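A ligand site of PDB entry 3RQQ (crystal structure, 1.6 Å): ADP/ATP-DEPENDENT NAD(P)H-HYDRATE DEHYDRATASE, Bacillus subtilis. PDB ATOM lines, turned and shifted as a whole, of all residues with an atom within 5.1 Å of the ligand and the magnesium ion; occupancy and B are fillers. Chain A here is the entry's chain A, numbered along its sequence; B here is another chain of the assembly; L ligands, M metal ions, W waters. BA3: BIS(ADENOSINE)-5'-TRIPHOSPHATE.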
ATOM      1  N   ASP A 131      19.416 -17.294  -9.084  1.00  0.00           N
ATOM      2  CA  ASP A 131      19.100 -18.712  -9.251  1.00  0.00           C
ATOM      3  C   ASP A 131      20.176 -19.321 -10.132  1.00  0.00           C
ATOM      4  O   ASP A 131      20.903 -18.633 -10.869  1.00  0.00           O
ATOM      5  CB  ASP A 131      17.703 -18.874  -9.872  1.00  0.00           C
ATOM      6  CG  ASP A 131      17.214 -20.298  -9.946  1.00  0.00           C
ATOM      7  OD1 ASP A 131      17.632 -21.166  -9.156  1.00  0.00           O
ATOM      8  OD2 ASP A 131      16.419 -20.576 -10.867  1.00  0.00           O
ATOM      9  N   ALA A 132      20.272 -20.651 -10.047  1.00  0.00           N
ATOM     10  CA  ALA A 132      21.005 -21.447 -11.056  1.00  0.00           C
ATOM     11  C   ALA A 132      22.431 -20.954 -11.245  1.00  0.00           C
ATOM     12  O   ALA A 132      23.209 -20.906 -10.281  1.00  0.00           O
ATOM     13  CB  ALA A 132      20.175 -21.521 -12.341  1.00  0.00           C
ATOM     14  N   THR A 150      17.759 -18.874  -4.544  1.00  0.00           N
ATOM     15  CA  THR A 150      16.872 -20.021  -4.667  1.00  0.00           C
ATOM     16  C   THR A 150      17.599 -21.357  -4.973  1.00  0.00           C
ATOM     17  O   THR A 150      17.340 -22.037  -5.995  1.00  0.00           O
ATOM     18  CB  THR A 150      15.787 -19.769  -5.717  1.00  0.00           C
ATOM     19  OG1 THR A 150      16.358 -19.635  -7.025  1.00  0.00           O
ATOM     20  CG2 THR A 150      14.952 -18.499  -5.410  1.00  0.00           C
ATOM     21  N   HIS A 152      18.794 -25.288  -4.959  1.00  0.00           N
ATOM     22  CA  HIS A 152      18.608 -26.686  -4.564  1.00  0.00           C
ATOM     23  C   HIS A 152      19.784 -27.117  -3.695  1.00  0.00           C
ATOM     24  O   HIS A 152      20.774 -26.403  -3.545  1.00  0.00           O
ATOM     25  CB  HIS A 152      18.318 -27.612  -5.726  1.00  0.00           C
ATOM     26  CG  HIS A 152      19.428 -27.867  -6.673  1.00  0.00           C
ATOM     27  ND1 HIS A 152      20.686 -28.288  -6.290  1.00  0.00           N
ATOM     28  CD2 HIS A 152      19.426 -27.895  -8.033  1.00  0.00           C
ATOM     29  CE1 HIS A 152      21.424 -28.515  -7.371  1.00  0.00           C
ATOM     30  NE2 HIS A 152      20.691 -28.275  -8.442  1.00  0.00           N
ATOM     31  N   GLU A 155      23.280 -26.728  -5.033  1.00  0.00           N
ATOM     32  CA  GLU A 155      23.675 -25.326  -5.183  1.00  0.00           C
ATOM     33  C   GLU A 155      23.990 -24.732  -3.795  1.00  0.00           C
ATOM     34  O   GLU A 155      24.859 -23.887  -3.675  1.00  0.00           O
ATOM     35  CB  GLU A 155      22.600 -24.522  -5.903  1.00  0.00           C
ATOM     36  CG  GLU A 155      22.434 -24.943  -7.366  1.00  0.00           C
ATOM     37  CD  GLU A 155      21.156 -24.565  -8.045  1.00  0.00           C
ATOM     38  OE1 GLU A 155      20.140 -24.421  -7.359  1.00  0.00           O
ATOM     39  OE2 GLU A 155      21.147 -24.487  -9.309  1.00  0.00           O
ATOM     40  N   LYS A 189      15.262 -25.310  -1.741  1.00  0.00           N
ATOM     41  CA  LYS A 189      14.291 -26.171  -2.392  1.00  0.00           C
ATOM     42  C   LYS A 189      14.339 -27.616  -1.908  1.00  0.00           C
ATOM     43  O   LYS A 189      15.358 -28.076  -1.313  1.00  0.00           O
ATOM     44  CB  LYS A 189      14.560 -26.103  -3.872  1.00  0.00           C
ATOM     45  CG  LYS A 189      14.268 -24.790  -4.444  1.00  0.00           C
ATOM     46  CD  LYS A 189      14.979 -24.668  -5.893  1.00  0.00           C
ATOM     47  CE  LYS A 189      14.459 -23.574  -6.705  1.00  0.00           C
ATOM     48  NZ  LYS A 189      15.396 -23.274  -7.877  1.00  0.00           N
ATOM     49  N   GLY A 190      13.232 -28.287  -2.132  1.00  0.00           N
ATOM     50  CA  GLY A 190      13.047 -29.693  -1.803  1.00  0.00           C
ATOM     51  C   GLY A 190      11.618 -29.901  -1.300  1.00  0.00           C
ATOM     52  O   GLY A 190      10.824 -28.953  -1.199  1.00  0.00           O
ATOM     53  N   ASN A 191      11.320 -31.120  -0.931  1.00  0.00           N
ATOM     54  CA  ASN A 191      10.110 -31.348  -0.156  1.00  0.00           C
ATOM     55  C   ASN A 191      10.255 -30.450   1.092  1.00  0.00           C
ATOM     56  O   ASN A 191      11.312 -30.325   1.641  1.00  0.00           O
ATOM     57  CB  ASN A 191      10.007 -32.822   0.235  1.00  0.00           C
ATOM     58  CG  ASN A 191       8.781 -33.110   1.114  1.00  0.00           C
ATOM     59  OD1 ASN A 191       7.681 -32.702   0.812  1.00  0.00           O
ATOM     60  ND2 ASN A 191       8.986 -33.833   2.209  1.00  0.00           N
ATOM     61  N   THR A 193      10.111 -27.121   1.176  1.00  0.00           N
ATOM     62  CA  THR A 193      11.033 -26.022   0.864  1.00  0.00           C
ATOM     63  C   THR A 193      11.095 -25.054   2.072  1.00  0.00           C
ATOM     64  O   THR A 193      10.062 -24.729   2.688  1.00  0.00           O
ATOM     65  CB  THR A 193      10.549 -25.265  -0.364  1.00  0.00           C
ATOM     66  OG1 THR A 193      10.794 -26.083  -1.531  1.00  0.00           O
ATOM     67  CG2 THR A 193      11.190 -23.852  -0.539  1.00  0.00           C
ATOM     68  N   THR A 207       3.109 -27.163   0.390  1.00  0.00           N
ATOM     69  CA  THR A 207       2.529 -27.642  -0.865  1.00  0.00           C
ATOM     70  C   THR A 207       3.584 -28.293  -1.746  1.00  0.00           C
ATOM     71  O   THR A 207       4.780 -28.032  -1.633  1.00  0.00           O
ATOM     72  CB  THR A 207       1.851 -26.498  -1.630  1.00  0.00           C
ATOM     73  OG1 THR A 207       2.850 -25.545  -1.979  1.00  0.00           O
ATOM     74  CG2 THR A 207       0.695 -25.854  -0.826  1.00  0.00           C
ATOM     75  N   GLY A 208       3.119 -29.011  -2.753  1.00  0.00           N
ATOM     76  CA  GLY A 208       3.954 -29.659  -3.683  1.00  0.00           C
ATOM     77  C   GLY A 208       4.062 -31.155  -3.484  1.00  0.00           C
ATOM     78  O   GLY A 208       3.648 -31.738  -2.467  1.00  0.00           O
ATOM     79  N   ASN A 209       4.669 -31.794  -4.472  1.00  0.00           N
ATOM     80  CA  ASN A 209       4.857 -33.227  -4.477  1.00  0.00           C
ATOM     81  C   ASN A 209       5.910 -33.609  -5.474  1.00  0.00           C
ATOM     82  O   ASN A 209       6.565 -32.719  -6.090  1.00  0.00           O
ATOM     83  CB  ASN A 209       3.540 -33.966  -4.733  1.00  0.00           C
ATOM     84  CG  ASN A 209       2.922 -33.589  -6.047  1.00  0.00           C
ATOM     85  OD1 ASN A 209       3.617 -33.478  -7.063  1.00  0.00           O
ATOM     86  ND2 ASN A 209       1.577 -33.376  -6.052  1.00  0.00           N
ATOM     87  N   GLY A 210       6.125 -34.919  -5.632  1.00  0.00           N
ATOM     88  CA  GLY A 210       7.182 -35.395  -6.511  1.00  0.00           C
ATOM     89  C   GLY A 210       7.042 -35.090  -7.977  1.00  0.00           C
ATOM     90  O   GLY A 210       8.004 -35.277  -8.763  1.00  0.00           O
ATOM     91  N   LEU A 212       7.116 -32.321  -9.079  1.00  0.00           N
ATOM     92  CA  LEU A 212       8.077 -31.200  -9.244  1.00  0.00           C
ATOM     93  C   LEU A 212       9.523 -31.628  -9.403  1.00  0.00           C
ATOM     94  O   LEU A 212      10.375 -30.815  -9.778  1.00  0.00           O
ATOM     95  CB  LEU A 212       7.964 -30.230  -8.071  1.00  0.00           C
ATOM     96  CG  LEU A 212       6.642 -29.486  -7.882  1.00  0.00           C
ATOM     97  CD1 LEU A 212       6.617 -28.732  -6.535  1.00  0.00           C
ATOM     98  CD2 LEU A 212       6.385 -28.533  -9.058  1.00  0.00           C
ATOM     99  N   ALA A 213       9.822 -32.900  -9.155  1.00  0.00           N
ATOM    100  CA  ALA A 213      11.194 -33.399  -9.189  1.00  0.00           C
ATOM    101  C   ALA A 213      11.583 -33.723 -10.629  1.00  0.00           C
ATOM    102  O   ALA A 213      11.818 -34.905 -10.972  1.00  0.00           O
ATOM    103  CB  ALA A 213      11.323 -34.652  -8.275  1.00  0.00           C
ATOM    104  N   LYS A 214      11.666 -32.699 -11.456  1.00  0.00           N
ATOM    105  CA  LYS A 214      11.971 -32.836 -12.868  1.00  0.00           C
ATOM    106  C   LYS A 214      12.491 -31.508 -13.350  1.00  0.00           C
ATOM    107  O   LYS A 214      12.063 -30.431 -12.863  1.00  0.00           O
ATOM    108  CB  LYS A 214      10.752 -33.284 -13.667  1.00  0.00           C
ATOM    109  CG  LYS A 214      11.060 -33.681 -15.082  1.00  0.00           C
ATOM    110  CD  LYS A 214       9.818 -34.111 -15.932  1.00  0.00           C
ATOM    111  CE  LYS A 214       9.047 -35.323 -15.336  1.00  0.00           C
ATOM    112  NZ  LYS A 214       7.711 -35.546 -16.036  1.00  0.00           N
ATOM    113  N   GLY A 215      13.405 -31.565 -14.335  1.00  0.00           N
ATOM    114  CA  GLY A 215      13.942 -30.368 -14.888  1.00  0.00           C
ATOM    115  C   GLY A 215      12.956 -29.307 -15.293  1.00  0.00           C
ATOM    116  O   GLY A 215      11.970 -29.596 -16.007  1.00  0.00           O
ATOM    117  N   GLY A 216      13.258 -28.075 -14.903  1.00  0.00           N
ATOM    118  CA  GLY A 216      12.555 -26.890 -15.327  1.00  0.00           C
ATOM    119  C   GLY A 216      11.621 -26.314 -14.296  1.00  0.00           C
ATOM    120  O   GLY A 216      11.202 -25.141 -14.413  1.00  0.00           O
ATOM    121  N   THR A 217      11.246 -27.100 -13.292  1.00  0.00           N
ATOM    122  CA  THR A 217      10.267 -26.598 -12.366  1.00  0.00           C
ATOM    123  C   THR A 217      10.811 -25.462 -11.499  1.00  0.00           C
ATOM    124  O   THR A 217      10.058 -24.555 -11.051  1.00  0.00           O
ATOM    125  CB  THR A 217       9.691 -27.673 -11.467  1.00  0.00           C
ATOM    126  OG1 THR A 217      10.745 -28.263 -10.699  1.00  0.00           O
ATOM    127  CG2 THR A 217       8.968 -28.792 -12.302  1.00  0.00           C
ATOM    128  N   GLY A 218      12.128 -25.422 -11.283  1.00  0.00           N
ATOM    129  CA  GLY A 218      12.721 -24.326 -10.564  1.00  0.00           C
ATOM    130  C   GLY A 218      12.824 -23.066 -11.381  1.00  0.00           C
ATOM    131  O   GLY A 218      12.788 -21.955 -10.857  1.00  0.00           O
ATOM    132  N   ASP A 219      13.022 -23.192 -12.701  1.00  0.00           N
ATOM    133  CA  ASP A 219      13.008 -22.019 -13.587  1.00  0.00           C
ATOM    134  C   ASP A 219      11.645 -21.373 -13.533  1.00  0.00           C
ATOM    135  O   ASP A 219      11.503 -20.133 -13.478  1.00  0.00           O
ATOM    136  CB  ASP A 219      13.349 -22.459 -15.014  1.00  0.00           C
ATOM    137  CG  ASP A 219      14.722 -23.098 -15.133  1.00  0.00           C
ATOM    138  OD1 ASP A 219      15.630 -22.698 -14.404  1.00  0.00           O
ATOM    139  OD2 ASP A 219      14.820 -24.008 -16.021  1.00  0.00           O
ATOM    140  N   LEU A 221       9.512 -21.561 -11.034  1.00  0.00           N
ATOM    141  CA  LEU A 221       9.431 -20.898  -9.713  1.00  0.00           C
ATOM    142  C   LEU A 221      10.128 -19.527  -9.707  1.00  0.00           C
ATOM    143  O   LEU A 221       9.597 -18.556  -9.209  1.00  0.00           O
ATOM    144  CB  LEU A 221       9.986 -21.781  -8.605  1.00  0.00           C
ATOM    145  CG  LEU A 221      10.042 -21.119  -7.210  1.00  0.00           C
ATOM    146  CD1 LEU A 221       8.616 -20.801  -6.765  1.00  0.00           C
ATOM    147  CD2 LEU A 221      10.733 -22.034  -6.200  1.00  0.00           C
ATOM    148  N   HIS A 246       3.189 -22.322  -6.457  1.00  0.00           N
ATOM    149  CA  HIS A 246       3.928 -23.237  -7.296  1.00  0.00           C
ATOM    150  C   HIS A 246       3.679 -24.681  -6.892  1.00  0.00           C
ATOM    151  O   HIS A 246       3.348 -25.542  -7.723  1.00  0.00           O
ATOM    152  CB  HIS A 246       5.403 -22.822  -7.209  1.00  0.00           C
ATOM    153  CG  HIS A 246       6.386 -23.700  -7.932  1.00  0.00           C
ATOM    154  ND1 HIS A 246       7.134 -24.654  -7.267  1.00  0.00           N
ATOM    155  CD2 HIS A 246       6.825 -23.694  -9.232  1.00  0.00           C
ATOM    156  CE1 HIS A 246       7.980 -25.216  -8.148  1.00  0.00           C
ATOM    157  NE2 HIS A 246       7.815 -24.649  -9.329  1.00  0.00           N
ATOM    158  N   ASP B  22       7.653 -40.654  -4.825  1.00  0.00           N
ATOM    159  CA  ASP B  22       7.439 -40.232  -3.439  1.00  0.00           C
ATOM    160  C   ASP B  22       7.780 -38.760  -3.174  1.00  0.00           C
ATOM    161  O   ASP B  22       8.597 -38.163  -3.891  1.00  0.00           O
ATOM    162  CB  ASP B  22       8.220 -41.150  -2.481  1.00  0.00           C
ATOM    163  CG  ASP B  22       9.721 -40.892  -2.530  1.00  0.00           C
ATOM    164  OD1 ASP B  22      10.347 -40.817  -1.459  1.00  0.00           O
ATOM    165  OD2 ASP B  22      10.265 -40.749  -3.668  1.00  0.00           O
ATOM    166  N   ALA B  23       7.192 -38.224  -2.108  1.00  0.00           N
ATOM    167  CA  ALA B  23       7.360 -36.816  -1.699  1.00  0.00           C
ATOM    168  C   ALA B  23       8.817 -36.481  -1.397  1.00  0.00           C
ATOM    169  O   ALA B  23       9.257 -35.352  -1.633  1.00  0.00           O
ATOM    170  CB  ALA B  23       6.491 -36.525  -0.451  1.00  0.00           C
ATOM    171  N   GLU B  24       9.550 -37.468  -0.864  1.00  0.00           N
ATOM    172  CA  GLU B  24      10.979 -37.335  -0.522  1.00  0.00           C
ATOM    173  C   GLU B  24      11.908 -37.544  -1.742  1.00  0.00           C
ATOM    174  O   GLU B  24      12.987 -38.164  -1.605  1.00  0.00           O
ATOM    175  CB  GLU B  24      11.353 -38.381   0.570  1.00  0.00           C
ATOM    176  CG  GLU B  24      11.177 -37.929   1.998  1.00  0.00           C
ATOM    177  CD  GLU B  24       9.784 -37.430   2.294  1.00  0.00           C
ATOM    178  OE1 GLU B  24       9.639 -36.205   2.503  1.00  0.00           O
ATOM    179  OE2 GLU B  24       8.847 -38.264   2.315  1.00  0.00           O
ATOM    180  N   SER B  25      11.494 -37.089  -2.923  1.00  0.00           N
ATOM    181  CA  SER B  25      12.302 -37.249  -4.137  1.00  0.00           C
ATOM    182  C   SER B  25      12.799 -35.932  -4.730  1.00  0.00           C
ATOM    183  O   SER B  25      12.187 -34.865  -4.532  1.00  0.00           O
ATOM    184  CB  SER B  25      11.545 -38.061  -5.209  1.00  0.00           C
ATOM    185  OG  SER B  25      10.243 -37.560  -5.493  1.00  0.00           O
ATOM    186  N   HIS B  26      13.943 -36.023  -5.411  1.00  0.00           N
ATOM    187  CA  HIS B  26      14.498 -34.897  -6.167  1.00  0.00           C
ATOM    188  C   HIS B  26      14.770 -35.395  -7.580  1.00  0.00           C
ATOM    189  O   HIS B  26      14.724 -36.627  -7.836  1.00  0.00           O
ATOM    190  CB  HIS B  26      15.753 -34.296  -5.488  1.00  0.00           C
ATOM    191  CG  HIS B  26      16.893 -35.255  -5.300  1.00  0.00           C
ATOM    192  ND1 HIS B  26      18.140 -35.051  -5.855  1.00  0.00           N
ATOM    193  CD2 HIS B  26      16.976 -36.422  -4.607  1.00  0.00           C
ATOM    194  CE1 HIS B  26      18.945 -36.052  -5.522  1.00  0.00           C
ATOM    195  NE2 HIS B  26      18.257 -36.908  -4.775  1.00  0.00           N
ATOM    196  N   LYS B  27      15.014 -34.483  -8.528  1.00  0.00           N
ATOM    197  CA  LYS B  27      15.153 -34.937  -9.939  1.00  0.00           C
ATOM    198  C   LYS B  27      16.298 -35.949 -10.136  1.00  0.00           C
ATOM    199  O   LYS B  27      16.194 -36.878 -10.948  1.00  0.00           O
ATOM    200  CB  LYS B  27      15.252 -33.753 -10.937  1.00  0.00           C
ATOM    201  CG  LYS B  27      16.409 -32.816 -10.760  1.00  0.00           C
ATOM    202  CD  LYS B  27      16.117 -31.461 -11.435  1.00  0.00           C
ATOM    203  CE  LYS B  27      16.647 -30.354 -10.588  1.00  0.00           C
ATOM    204  NZ  LYS B  27      15.902 -30.356  -9.297  1.00  0.00           N
HETATM  205  N9A BA3 L   1      10.596 -30.016  -5.819  1.00  0.00           N
HETATM  206  C8A BA3 L   1      11.407 -31.012  -6.301  1.00  0.00           C
HETATM  207  N7A BA3 L   1      11.046 -32.200  -5.728  1.00  0.00           N
HETATM  208  C5A BA3 L   1       9.991 -31.947  -4.898  1.00  0.00           C
HETATM  209  C6A BA3 L   1       9.237 -32.766  -4.074  1.00  0.00           C
HETATM  210  N6A BA3 L   1       9.539 -34.046  -3.996  1.00  0.00           N
HETATM  211  N1A BA3 L   1       8.222 -32.199  -3.300  1.00  0.00           N
HETATM  212  C2A BA3 L   1       7.927 -30.862  -3.375  1.00  0.00           C
HETATM  213  N3A BA3 L   1       8.689 -30.028  -4.196  1.00  0.00           N
HETATM  214  C4A BA3 L   1       9.708 -30.578  -4.931  1.00  0.00           C
HETATM  215  O5B BA3 L   1      13.761 -26.652  -8.704  1.00  0.00           O
HETATM  216  C5B BA3 L   1      13.037 -27.821  -8.382  1.00  0.00           C
HETATM  217  C4B BA3 L   1      11.689 -27.333  -7.865  1.00  0.00           C
HETATM  218  O4B BA3 L   1      10.936 -28.521  -7.604  1.00  0.00           O
HETATM  219  C3B BA3 L   1      11.782 -26.666  -6.466  1.00  0.00           C
HETATM  220  O3B BA3 L   1      10.749 -25.720  -6.301  1.00  0.00           O
HETATM  221  C2B BA3 L   1      11.664 -27.804  -5.473  1.00  0.00           C
HETATM  222  O2B BA3 L   1      11.334 -27.468  -4.133  1.00  0.00           O
HETATM  223  C1B BA3 L   1      10.607 -28.600  -6.195  1.00  0.00           C
HETATM  224  PE  BA3 L   1      15.247 -26.849  -9.248  1.00  0.00           P
HETATM  225  O1E BA3 L   1      16.110 -27.871  -8.547  1.00  0.00           O
HETATM  226  O2E BA3 L   1      15.910 -25.467  -9.401  1.00  0.00           O
HETATM  227  O3E BA3 L   1      14.839 -27.357 -10.790  1.00  0.00           O
HETATM  228  PF  BA3 L   1      15.397 -26.810 -12.252  1.00  0.00           P
HETATM  229  O1F BA3 L   1      14.401 -25.985 -12.968  1.00  0.00           O
HETATM  230  O2F BA3 L   1      15.776 -28.064 -13.062  1.00  0.00           O
HETATM  231  O3F BA3 L   1      16.701 -25.942 -11.961  1.00  0.00           O
HETATM  232 MG    MG M   1      17.347 -24.780 -10.578  1.00  0.00          MG
HETATM  233  O   HOH W   1      10.003 -24.779  -3.994  1.00  0.00           O
HETATM  234  O   HOH W   2       8.624 -27.247  -3.581  1.00  0.00           O
HETATM  235  O   HOH W   3      16.238 -23.102 -11.593  1.00  0.00           O
HETATM  236  O   HOH W   4      14.283 -31.618  -7.941  1.00  0.00           O
HETATM  237  O   HOH W   5      19.264 -24.941 -13.352  1.00  0.00           O
HETATM  238  O   HOH W   6      17.892 -23.697  -8.954  1.00  0.00           O
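Merely in contact with the magnesium ion: Asp 131 and Lys 189. Of the 29 residues printed, 2 come within 4 Å of the magnesium ion. The nearest printed residue that does not touch the magnesium ion is Glu 155 (4.02 Å).
Water W3 bridges OD2 of Asp 131 (2.6 Å) and OD1 of Asp 219 (2.9 Å). Water W1 bridges an oxygen (O3B) of the ligand (2.6 Å) and the side-chain hydroxyl (OG1) of Thr 193 (2.9 Å). Water W2 lies within hydrogen-bond range of an oxygen (O2B) of the ligand and the side-chain hydroxyl of Thr 193.
The backbone NH (N) of Gly 218 is in hydrogen-bond range of an oxygen (O1F) of the ligand, 2.9 Å away. The backbone NH (N) of Thr 217 lies within hydrogen-bond range of an oxygen (O1F) of the ligand. An oxygen (O2B) of the ligand sits at hydrogen-bond distance from the backbone NH of Gly 190 (2.9 Å). An oxygen (O4B) of the ligand lies within hydrogen-bond range of the side-chain hydroxyl of Thr 217 (3.1 Å). O2B of the ligand sits at hydrogen-bond distance from O of Gly 190 (3.3 Å). O1E of the ligand lies within salt-bridge range of NZ of Lys 27 of chain B, 2.6 Å away. An oxygen (O2B) of the ligand lies within hydrogen-bond range of the side-chain hydroxyl (OG1) of Thr 193 (3.0 Å). N of Gly 216 is in hydrogen-bond range of O1F of the ligand (3.1 Å). O of Ser 25 of chain B sits at hydrogen-bond distance from N6A of the ligand, at 2.8 Å. O of Ala 23 of chain B sits at hydrogen-bond distance from N6A of the ligand (2.7 Å). The side-chain amino group (NZ) of Lys 189 sits close to an oxygen (O2E) of the ligand, at 2.7 Å. The backbone NH of Asp 219 lies within hydrogen-bond range of an oxygen (O1F) of the ligand (3.1 Å).
The side-chain carboxylate of Glu 24 of chain B is in hydrogen-bond range of the side-chain amide nitrogen of Asn 191 (2.5 Å). The backbone carbonyl oxygen of Leu 212 sits at hydrogen-bond distance from the side-chain hydroxyl of Thr 217, 2.7 Å away. The side-chain amino group of Lys 189 is in hydrogen-bond range of the backbone carbonyl oxygen of Thr 150, 3.0 Å away. The side-chain amino group (NZ) of Lys 189 lies within salt-bridge range of the side-chain carboxylate (OD1) of Asp 131 (3.3 Å). The side-chain carboxylate (OD1) of Asp 131 sits at hydrogen-bond distance from the side-chain hydroxyl (OG1) of Thr 150. The side-chain carboxylate (OE1) of Glu 155 lies within hydrogen-bond range of the backbone NH (N) of His 152, 2.9 Å away. The backbone carbonyl oxygen (O) of Thr 217 is in hydrogen-bond range of a ring nitrogen (NE2) of His 246 (2.8 Å). OG1 of Thr 217 sits at hydrogen-bond distance from O of Lys 214.
A nitrogen (N1A) of the ligand sits close to the backbone carbonyl oxygen (O) of Asn 209, at 3.3 Å. O of Leu 212 sits close to O4B of the ligand, at 3.2 Å. Residues that only touch the ligand: His 152 (3.4 Å), His 246 (3.4 Å), Gly 215 (3.5 Å), Ala 213 (3.5 Å), Leu 221 (3.7 Å), Gly 210 (3.7 Å), Asn 191 (3.8 Å) and Gly 208 (3.9 Å). Hydrophobic or aromatic side chains that line the ligand: His 152, Leu 212, Ala 213, Leu 221 and His 246. Within 4 Å of the ligand: His 152, Lys 189, Gly 190, Asn 191, Thr 193, Gly 208, Asn 209, Gly 210, Leu 212, Ala 213, Gly 215, Gly 216, Thr 217, Gly 218, Asp 219, Leu 221, His 246, Ala 23 of chain B, Ser 25 of chain B and Lys 27 of chain B.
O3F of the ligand is bound to the magnesium ion (1.9 Å). An oxygen (O2E) of the ligand binds the magnesium ion, 2.0 Å away. The magnesium ion is bound by water W6 (2.0 Å). Water W3 binds the magnesium ion, 2.3 Å away. The magnesium ion has four donor atoms within binding distance.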
